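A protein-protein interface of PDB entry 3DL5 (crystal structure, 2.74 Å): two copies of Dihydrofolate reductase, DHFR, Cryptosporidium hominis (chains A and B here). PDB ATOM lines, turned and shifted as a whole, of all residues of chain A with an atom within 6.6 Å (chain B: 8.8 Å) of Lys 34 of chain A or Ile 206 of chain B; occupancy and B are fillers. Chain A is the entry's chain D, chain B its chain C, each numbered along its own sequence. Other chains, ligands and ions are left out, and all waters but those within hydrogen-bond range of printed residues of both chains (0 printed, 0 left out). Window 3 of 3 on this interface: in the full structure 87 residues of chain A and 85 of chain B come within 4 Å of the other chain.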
ATOM      1  N   ILE A  29     -37.516  18.004 -30.900  1.00  0.00           N
ATOM      2  CA  ILE A  29     -36.191  18.343 -30.393  1.00  0.00           C
ATOM      3  C   ILE A  29     -36.176  19.700 -29.726  1.00  0.00           C
ATOM      4  O   ILE A  29     -36.104  20.747 -30.370  1.00  0.00           O
ATOM      5  CB  ILE A  29     -35.119  18.307 -31.515  1.00  0.00           C
ATOM      6  CG1 ILE A  29     -35.101  16.923 -32.176  1.00  0.00           C
ATOM      7  CG2 ILE A  29     -33.744  18.585 -30.931  1.00  0.00           C
ATOM      8  CD1 ILE A  29     -34.136  16.807 -33.348  1.00  0.00           C
ATOM      9  N   SER A  30     -36.243  19.658 -28.409  1.00  0.00           N
ATOM     10  CA  SER A  30     -36.251  20.843 -27.577  1.00  0.00           C
ATOM     11  C   SER A  30     -35.153  21.855 -27.937  1.00  0.00           C
ATOM     12  O   SER A  30     -35.435  23.026 -28.217  1.00  0.00           O
ATOM     13  CB  SER A  30     -36.114  20.396 -26.119  1.00  0.00           C
ATOM     14  OG  SER A  30     -36.064  21.497 -25.241  1.00  0.00           O
ATOM     15  N   GLU A  31     -33.904  21.401 -27.924  1.00  0.00           N
ATOM     16  CA  GLU A  31     -32.779  22.277 -28.224  1.00  0.00           C
ATOM     17  C   GLU A  31     -32.925  23.043 -29.535  1.00  0.00           C
ATOM     18  O   GLU A  31     -32.537  24.213 -29.622  1.00  0.00           O
ATOM     19  CB  GLU A  31     -31.469  21.483 -28.248  1.00  0.00           C
ATOM     20  CG  GLU A  31     -31.065  20.872 -26.916  1.00  0.00           C
ATOM     21  CD  GLU A  31     -31.710  19.528 -26.663  1.00  0.00           C
ATOM     22  OE1 GLU A  31     -31.316  18.858 -25.686  1.00  0.00           O
ATOM     23  OE2 GLU A  31     -32.604  19.135 -27.439  1.00  0.00           O
ATOM     24  N   ASP A  32     -33.476  22.392 -30.556  1.00  0.00           N
ATOM     25  CA  ASP A  32     -33.646  23.051 -31.843  1.00  0.00           C
ATOM     26  C   ASP A  32     -34.610  24.227 -31.742  1.00  0.00           C
ATOM     27  O   ASP A  32     -34.386  25.274 -32.355  1.00  0.00           O
ATOM     28  CB  ASP A  32     -34.134  22.061 -32.900  1.00  0.00           C
ATOM     29  CG  ASP A  32     -34.405  22.724 -34.242  1.00  0.00           C
ATOM     30  OD1 ASP A  32     -33.545  23.493 -34.714  1.00  0.00           O
ATOM     31  OD2 ASP A  32     -35.475  22.464 -34.828  1.00  0.00           O
ATOM     32  N   LEU A  33     -35.681  24.068 -30.974  1.00  0.00           N
ATOM     33  CA  LEU A  33     -36.614  25.166 -30.824  1.00  0.00           C
ATOM     34  C   LEU A  33     -35.916  26.293 -30.086  1.00  0.00           C
ATOM     35  O   LEU A  33     -36.055  27.466 -30.448  1.00  0.00           O
ATOM     36  CB  LEU A  33     -37.859  24.725 -30.061  1.00  0.00           C
ATOM     37  CG  LEU A  33     -38.840  23.850 -30.842  1.00  0.00           C
ATOM     38  CD1 LEU A  33     -40.056  23.634 -29.957  1.00  0.00           C
ATOM     39  CD2 LEU A  33     -39.245  24.508 -32.177  1.00  0.00           C
ATOM     40  N   LYS A  34     -35.157  25.944 -29.052  1.00  0.00           N
ATOM     41  CA  LYS A  34     -34.428  26.957 -28.298  1.00  0.00           C
ATOM     42  C   LYS A  34     -33.533  27.721 -29.272  1.00  0.00           C
ATOM     43  O   LYS A  34     -33.332  28.929 -29.129  1.00  0.00           O
ATOM     44  CB  LYS A  34     -33.586  26.310 -27.196  1.00  0.00           C
ATOM     45  CG  LYS A  34     -34.063  26.634 -25.792  1.00  0.00           C
ATOM     46  CD  LYS A  34     -33.000  27.405 -25.014  1.00  0.00           C
ATOM     47  CE  LYS A  34     -33.452  27.731 -23.586  1.00  0.00           C
ATOM     48  NZ  LYS A  34     -32.381  28.423 -22.791  1.00  0.00           N
ATOM     49  N   PHE A  35     -33.007  27.011 -30.271  1.00  0.00           N
ATOM     50  CA  PHE A  35     -32.154  27.643 -31.272  1.00  0.00           C
ATOM     51  C   PHE A  35     -33.001  28.641 -32.055  1.00  0.00           C
ATOM     52  O   PHE A  35     -32.695  29.841 -32.113  1.00  0.00           O
ATOM     53  CB  PHE A  35     -31.575  26.604 -32.237  1.00  0.00           C
ATOM     54  CG  PHE A  35     -30.609  27.184 -33.232  1.00  0.00           C
ATOM     55  CD1 PHE A  35     -29.407  27.736 -32.808  1.00  0.00           C
ATOM     56  CD2 PHE A  35     -30.922  27.225 -34.586  1.00  0.00           C
ATOM     57  CE1 PHE A  35     -28.529  28.326 -33.717  1.00  0.00           C
ATOM     58  CE2 PHE A  35     -30.054  27.813 -35.500  1.00  0.00           C
ATOM     59  CZ  PHE A  35     -28.856  28.366 -35.062  1.00  0.00           C
ATOM     60  N   PHE A  36     -34.071  28.127 -32.653  1.00  0.00           N
ATOM     61  CA  PHE A  36     -34.984  28.953 -33.427  1.00  0.00           C
ATOM     62  C   PHE A  36     -35.324  30.209 -32.649  1.00  0.00           C
ATOM     63  O   PHE A  36     -35.302  31.314 -33.194  1.00  0.00           O
ATOM     64  CB  PHE A  36     -36.270  28.178 -33.738  1.00  0.00           C
ATOM     65  CG  PHE A  36     -37.350  29.021 -34.350  1.00  0.00           C
ATOM     66  CD1 PHE A  36     -38.121  29.871 -33.562  1.00  0.00           C
ATOM     67  CD2 PHE A  36     -37.573  28.994 -35.716  1.00  0.00           C
ATOM     68  CE1 PHE A  36     -39.090  30.680 -34.133  1.00  0.00           C
ATOM     69  CE2 PHE A  36     -38.540  29.798 -36.293  1.00  0.00           C
ATOM     70  CZ  PHE A  36     -39.298  30.641 -35.503  1.00  0.00           C
ATOM     71  N   SER A  37     -35.637  30.035 -31.370  1.00  0.00           N
ATOM     72  CA  SER A  37     -35.993  31.164 -30.528  1.00  0.00           C
ATOM     73  C   SER A  37     -34.839  32.137 -30.358  1.00  0.00           C
ATOM     74  O   SER A  37     -35.022  33.348 -30.472  1.00  0.00           O
ATOM     75  CB  SER A  37     -36.461  30.682 -29.156  1.00  0.00           C
ATOM     76  OG  SER A  37     -36.801  31.786 -28.336  1.00  0.00           O
ATOM     77  N   LYS A  38     -33.646  31.614 -30.091  1.00  0.00           N
ATOM     78  CA  LYS A  38     -32.495  32.488 -29.898  1.00  0.00           C
ATOM     79  C   LYS A  38     -32.050  33.195 -31.165  1.00  0.00           C
ATOM     80  O   LYS A  38     -31.757  34.389 -31.151  1.00  0.00           O
ATOM     81  CB  LYS A  38     -31.315  31.711 -29.310  1.00  0.00           C
ATOM     82  CG  LYS A  38     -31.472  31.420 -27.849  1.00  0.00           C
ATOM     83  CD  LYS A  38     -30.214  30.817 -27.282  1.00  0.00           C
ATOM     84  CE  LYS A  38     -30.394  30.489 -25.803  1.00  0.00           C
ATOM     85  NZ  LYS A  38     -30.762  31.695 -25.012  1.00  0.00           N
ATOM     86  N   ILE A  39     -32.006  32.459 -32.265  1.00  0.00           N
ATOM     87  CA  ILE A  39     -31.574  33.052 -33.514  1.00  0.00           C
ATOM     88  C   ILE A  39     -32.550  34.127 -34.012  1.00  0.00           C
ATOM     89  O   ILE A  39     -32.117  35.203 -34.432  1.00  0.00           O
ATOM     90  CB  ILE A  39     -31.359  31.955 -34.602  1.00  0.00           C
ATOM     91  CG1 ILE A  39     -30.477  32.499 -35.724  1.00  0.00           C
ATOM     92  CG2 ILE A  39     -32.680  31.483 -35.156  1.00  0.00           C
ATOM     93  CD1 ILE A  39     -29.030  32.710 -35.310  1.00  0.00           C
ATOM     94  N   PHE A 172     -25.948  21.872 -36.860  1.00  0.00           N
ATOM     95  CA  PHE A 172     -26.345  23.183 -37.360  1.00  0.00           C
ATOM     96  C   PHE A 172     -25.427  23.743 -38.435  1.00  0.00           C
ATOM     97  O   PHE A 172     -24.209  23.792 -38.259  1.00  0.00           O
ATOM     98  CB  PHE A 172     -26.395  24.170 -36.201  1.00  0.00           C
ATOM     99  CG  PHE A 172     -27.349  23.777 -35.120  1.00  0.00           C
ATOM    100  CD1 PHE A 172     -28.700  24.061 -35.234  1.00  0.00           C
ATOM    101  CD2 PHE A 172     -26.895  23.115 -33.990  1.00  0.00           C
ATOM    102  CE1 PHE A 172     -29.589  23.690 -34.233  1.00  0.00           C
ATOM    103  CE2 PHE A 172     -27.767  22.741 -32.987  1.00  0.00           C
ATOM    104  CZ  PHE A 172     -29.121  23.029 -33.104  1.00  0.00           C
ATOM    105  N   THR B 199     -23.965  32.592 -33.961  1.00  0.00           N
ATOM    106  CA  THR B 199     -24.575  31.279 -33.972  1.00  0.00           C
ATOM    107  C   THR B 199     -23.865  30.348 -32.977  1.00  0.00           C
ATOM    108  O   THR B 199     -24.515  29.672 -32.173  1.00  0.00           O
ATOM    109  CB  THR B 199     -24.515  30.677 -35.382  1.00  0.00           C
ATOM    110  OG1 THR B 199     -25.413  31.390 -36.236  1.00  0.00           O
ATOM    111  CG2 THR B 199     -24.892  29.209 -35.360  1.00  0.00           C
ATOM    112  N   VAL B 200     -22.535  30.314 -33.027  1.00  0.00           N
ATOM    113  CA  VAL B 200     -21.769  29.460 -32.125  1.00  0.00           C
ATOM    114  C   VAL B 200     -21.999  29.861 -30.666  1.00  0.00           C
ATOM    115  O   VAL B 200     -22.137  28.995 -29.802  1.00  0.00           O
ATOM    116  CB  VAL B 200     -20.238  29.483 -32.480  1.00  0.00           C
ATOM    117  CG1 VAL B 200     -19.414  28.859 -31.362  1.00  0.00           C
ATOM    118  CG2 VAL B 200     -19.997  28.695 -33.772  1.00  0.00           C
ATOM    119  N   ASP B 201     -22.051  31.162 -30.394  1.00  0.00           N
ATOM    120  CA  ASP B 201     -22.295  31.636 -29.035  1.00  0.00           C
ATOM    121  C   ASP B 201     -23.640  31.142 -28.514  1.00  0.00           C
ATOM    122  O   ASP B 201     -23.725  30.577 -27.422  1.00  0.00           O
ATOM    123  CB  ASP B 201     -22.286  33.160 -28.984  1.00  0.00           C
ATOM    124  CG  ASP B 201     -20.891  33.726 -28.939  1.00  0.00           C
ATOM    125  OD1 ASP B 201     -20.754  34.966 -28.965  1.00  0.00           O
ATOM    126  OD2 ASP B 201     -19.935  32.926 -28.871  1.00  0.00           O
ATOM    127  N   LEU B 202     -24.687  31.372 -29.301  1.00  0.00           N
ATOM    128  CA  LEU B 202     -26.036  30.958 -28.946  1.00  0.00           C
ATOM    129  C   LEU B 202     -26.087  29.450 -28.761  1.00  0.00           C
ATOM    130  O   LEU B 202     -26.678  28.946 -27.804  1.00  0.00           O
ATOM    131  CB  LEU B 202     -27.017  31.381 -30.044  1.00  0.00           C
ATOM    132  CG  LEU B 202     -27.695  32.755 -29.950  1.00  0.00           C
ATOM    133  CD1 LEU B 202     -26.768  33.810 -29.362  1.00  0.00           C
ATOM    134  CD2 LEU B 202     -28.148  33.140 -31.346  1.00  0.00           C
ATOM    135  N   LEU B 203     -25.471  28.731 -29.686  1.00  0.00           N
ATOM    136  CA  LEU B 203     -25.433  27.286 -29.609  1.00  0.00           C
ATOM    137  C   LEU B 203     -24.728  26.907 -28.302  1.00  0.00           C
ATOM    138  O   LEU B 203     -25.012  25.870 -27.709  1.00  0.00           O
ATOM    139  CB  LEU B 203     -24.675  26.753 -30.816  1.00  0.00           C
ATOM    140  CG  LEU B 203     -25.297  25.634 -31.647  1.00  0.00           C
ATOM    141  CD1 LEU B 203     -26.796  25.795 -31.771  1.00  0.00           C
ATOM    142  CD2 LEU B 203     -24.631  25.645 -33.014  1.00  0.00           C
ATOM    143  N   GLY B 204     -23.820  27.774 -27.853  1.00  0.00           N
ATOM    144  CA  GLY B 204     -23.092  27.545 -26.618  1.00  0.00           C
ATOM    145  C   GLY B 204     -23.976  27.758 -25.401  1.00  0.00           C
ATOM    146  O   GLY B 204     -23.860  27.045 -24.403  1.00  0.00           O
ATOM    147  N   GLU B 205     -24.860  28.749 -25.477  1.00  0.00           N
ATOM    148  CA  GLU B 205     -25.789  29.044 -24.387  1.00  0.00           C
ATOM    149  C   GLU B 205     -26.780  27.899 -24.203  1.00  0.00           C
ATOM    150  O   GLU B 205     -27.095  27.502 -23.088  1.00  0.00           O
ATOM    151  CB  GLU B 205     -26.561  30.323 -24.685  1.00  0.00           C
ATOM    152  CG  GLU B 205     -25.780  31.587 -24.422  1.00  0.00           C
ATOM    153  CD  GLU B 205     -26.441  32.815 -25.021  1.00  0.00           C
ATOM    154  OE1 GLU B 205     -27.671  32.981 -24.836  1.00  0.00           O
ATOM    155  OE2 GLU B 205     -25.723  33.614 -25.670  1.00  0.00           O
ATOM    156  N   ILE B 206     -27.267  27.371 -25.313  1.00  0.00           N
ATOM    157  CA  ILE B 206     -28.218  26.282 -25.285  1.00  0.00           C
ATOM    158  C   ILE B 206     -27.653  24.989 -24.716  1.00  0.00           C
ATOM    159  O   ILE B 206     -28.284  24.354 -23.874  1.00  0.00           O
ATOM    160  CB  ILE B 206     -28.739  25.988 -26.704  1.00  0.00           C
ATOM    161  CG1 ILE B 206     -29.628  27.134 -27.174  1.00  0.00           C
ATOM    162  CG2 ILE B 206     -29.485  24.659 -26.731  1.00  0.00           C
ATOM    163  CD1 ILE B 206     -30.099  26.988 -28.603  1.00  0.00           C
ATOM    164  N   PHE B 207     -26.457  24.609 -25.165  1.00  0.00           N
ATOM    165  CA  PHE B 207     -25.841  23.345 -24.752  1.00  0.00           C
ATOM    166  C   PHE B 207     -24.873  23.291 -23.571  1.00  0.00           C
ATOM    167  O   PHE B 207     -24.587  22.208 -23.053  1.00  0.00           O
ATOM    168  CB  PHE B 207     -25.148  22.722 -25.963  1.00  0.00           C
ATOM    169  CG  PHE B 207     -26.096  22.190 -26.995  1.00  0.00           C
ATOM    170  CD1 PHE B 207     -26.774  20.991 -26.778  1.00  0.00           C
ATOM    171  CD2 PHE B 207     -26.297  22.875 -28.190  1.00  0.00           C
ATOM    172  CE1 PHE B 207     -27.640  20.475 -27.742  1.00  0.00           C
ATOM    173  CE2 PHE B 207     -27.156  22.375 -29.159  1.00  0.00           C
ATOM    174  CZ  PHE B 207     -27.831  21.169 -28.938  1.00  0.00           C
ATOM    175  N   GLY B 208     -24.352  24.432 -23.142  1.00  0.00           N
ATOM    176  CA  GLY B 208     -23.412  24.396 -22.037  1.00  0.00           C
ATOM    177  C   GLY B 208     -22.236  23.495 -22.367  1.00  0.00           C
ATOM    178  O   GLY B 208     -21.778  23.436 -23.516  1.00  0.00           O
ATOM    179  N   ILE B 209     -21.751  22.763 -21.375  1.00  0.00           N
ATOM    180  CA  ILE B 209     -20.611  21.898 -21.612  1.00  0.00           C
ATOM    181  C   ILE B 209     -20.913  20.662 -22.448  1.00  0.00           C
ATOM    182  O   ILE B 209     -20.091  19.745 -22.544  1.00  0.00           O
ATOM    183  CB  ILE B 209     -19.954  21.496 -20.298  1.00  0.00           C
ATOM    184  CG1 ILE B 209     -20.953  20.737 -19.434  1.00  0.00           C
ATOM    185  CG2 ILE B 209     -19.444  22.750 -19.587  1.00  0.00           C
ATOM    186  CD1 ILE B 209     -20.361  20.242 -18.148  1.00  0.00           C
ATOM    187  N   ARG B 210     -22.114  20.589 -22.992  1.00  0.00           N
ATOM    188  CA  ARG B 210     -22.452  19.517 -23.916  1.00  0.00           C
ATOM    189  C   ARG B 210     -21.878  19.806 -25.299  1.00  0.00           C
ATOM    190  O   ARG B 210     -21.848  18.940 -26.167  1.00  0.00           O
ATOM    191  CB  ARG B 210     -23.957  19.367 -24.000  1.00  0.00           C
ATOM    192  CG  ARG B 210     -24.568  18.817 -22.745  1.00  0.00           C
ATOM    193  CD  ARG B 210     -26.054  18.843 -22.878  1.00  0.00           C
ATOM    194  NE  ARG B 210     -26.468  18.175 -24.099  1.00  0.00           N
ATOM    195  CZ  ARG B 210     -27.679  18.295 -24.628  1.00  0.00           C
ATOM    196  NH1 ARG B 210     -28.585  19.066 -24.033  1.00  0.00           N
ATOM    197  NH2 ARG B 210     -27.982  17.641 -25.744  1.00  0.00           N
ATOM    198  N   LYS B 211     -21.434  21.044 -25.491  1.00  0.00           N
ATOM    199  CA  LYS B 211     -20.812  21.466 -26.743  1.00  0.00           C
ATOM    200  C   LYS B 211     -19.318  21.515 -26.444  1.00  0.00           C
ATOM    201  O   LYS B 211     -18.856  22.399 -25.715  1.00  0.00           O
ATOM    202  CB  LYS B 211     -21.315  22.851 -27.145  1.00  0.00           C
ATOM    203  CG  LYS B 211     -20.613  23.461 -28.331  1.00  0.00           C
ATOM    204  CD  LYS B 211     -21.409  24.652 -28.853  1.00  0.00           C
ATOM    205  CE  LYS B 211     -20.609  25.498 -29.843  1.00  0.00           C
ATOM    206  NZ  LYS B 211     -19.897  24.695 -30.874  1.00  0.00           N
ATOM    207  N   ASN B 214     -17.177  24.443 -25.500  1.00  0.00           N
ATOM    208  CA  ASN B 214     -17.224  25.066 -24.178  1.00  0.00           C
ATOM    209  C   ASN B 214     -16.269  24.393 -23.199  1.00  0.00           C
ATOM    210  O   ASN B 214     -15.964  24.944 -22.141  1.00  0.00           O
ATOM    211  CB  ASN B 214     -18.642  25.038 -23.596  1.00  0.00           C
ATOM    212  CG  ASN B 214     -19.522  26.156 -24.135  1.00  0.00           C
ATOM    213  OD1 ASN B 214     -19.063  27.275 -24.335  1.00  0.00           O
ATOM    214  ND2 ASN B 214     -20.799  25.862 -24.345  1.00  0.00           N
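Printed residues of chain B that touch a printed residue of chain A: Thr 199, Leu 202, Leu 203, Glu 205, Ile 206, Phe 207 and Arg 210.
Along chain A the printed residues that touch a printed residue of chain B span positions 31 to 172.
Among the printed residues, 12 pairs touch across the chains.
Lys 34 of chain A touches just one residue of chain B: Ile 206.
Printed residues of chain A within 4 Å of Arg 210 of chain B: Glu 31 (3.2 Å).
Printed residues of chain B within 4 Å of Phe 172 of chain A: Leu 203 (3.4 Å) and Phe 207 (3.9 Å).
Of the printed residues of chain A, Leu 202 of chain B touches Lys 38 (3.8 Å).
Of the printed residues of chain A, Phe 207 of chain B touches Glu 31 and Phe 172.
Printed residues of chain A within 4 Å of Leu 203 of chain B: Phe 35 (3.4 Å) and Phe 172 (3.4 Å).
Leu 33 of chain A touches none of the printed residues of chain B.
The nearest printed residue of chain B that does not touch Phe 35 of chain A is Thr 199 of chain B (4.1 Å).
O of Glu 31 of chain A touches CD1 of Ile 206 of chain B, 3.8 Å away.
Phe 207 of chain B touches Glu 31 of chain A (CE1 to CG, 3.5 Å).
Lys 34 of chain A touches Ile 206 of chain B.
Leu 203 of chain B touches Phe 35 of chain A (CD1 to CD1, 3.4 Å).
Ile 206 of chain B touches Phe 35 of chain A (CD1 to N, 3.4 Å).
Leu 202 of chain B touches Lys 38 of chain A.
CG1 of Ile 206 of chain B touches CE of Lys 38 of chain A, 3.7 Å away.
Ile 39 of chain A touches Thr 199 of chain B (CD1 to OG1, 3.96 Å).
Phe 172 of chain A touches Leu 203 of chain B.
CE2 of Phe 207 of chain B touches CE2 of Phe 172 of chain A (3.9 Å).
No position is printed for both chains.
Of the 12 pairs that touch across the chains among the printed residues, none has its exchanged pair printed and touching as well.
The side-chain carboxylate (OE1) of Glu 205 of chain B is in salt-bridge range of the side-chain amino group (NZ) of Lys 38 of chain A (3.4 Å).
The side-chain carboxylate of Glu 31 of chain A is in salt-bridge range of the guanidinium group of Arg 210 of chain B (3.2 Å).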
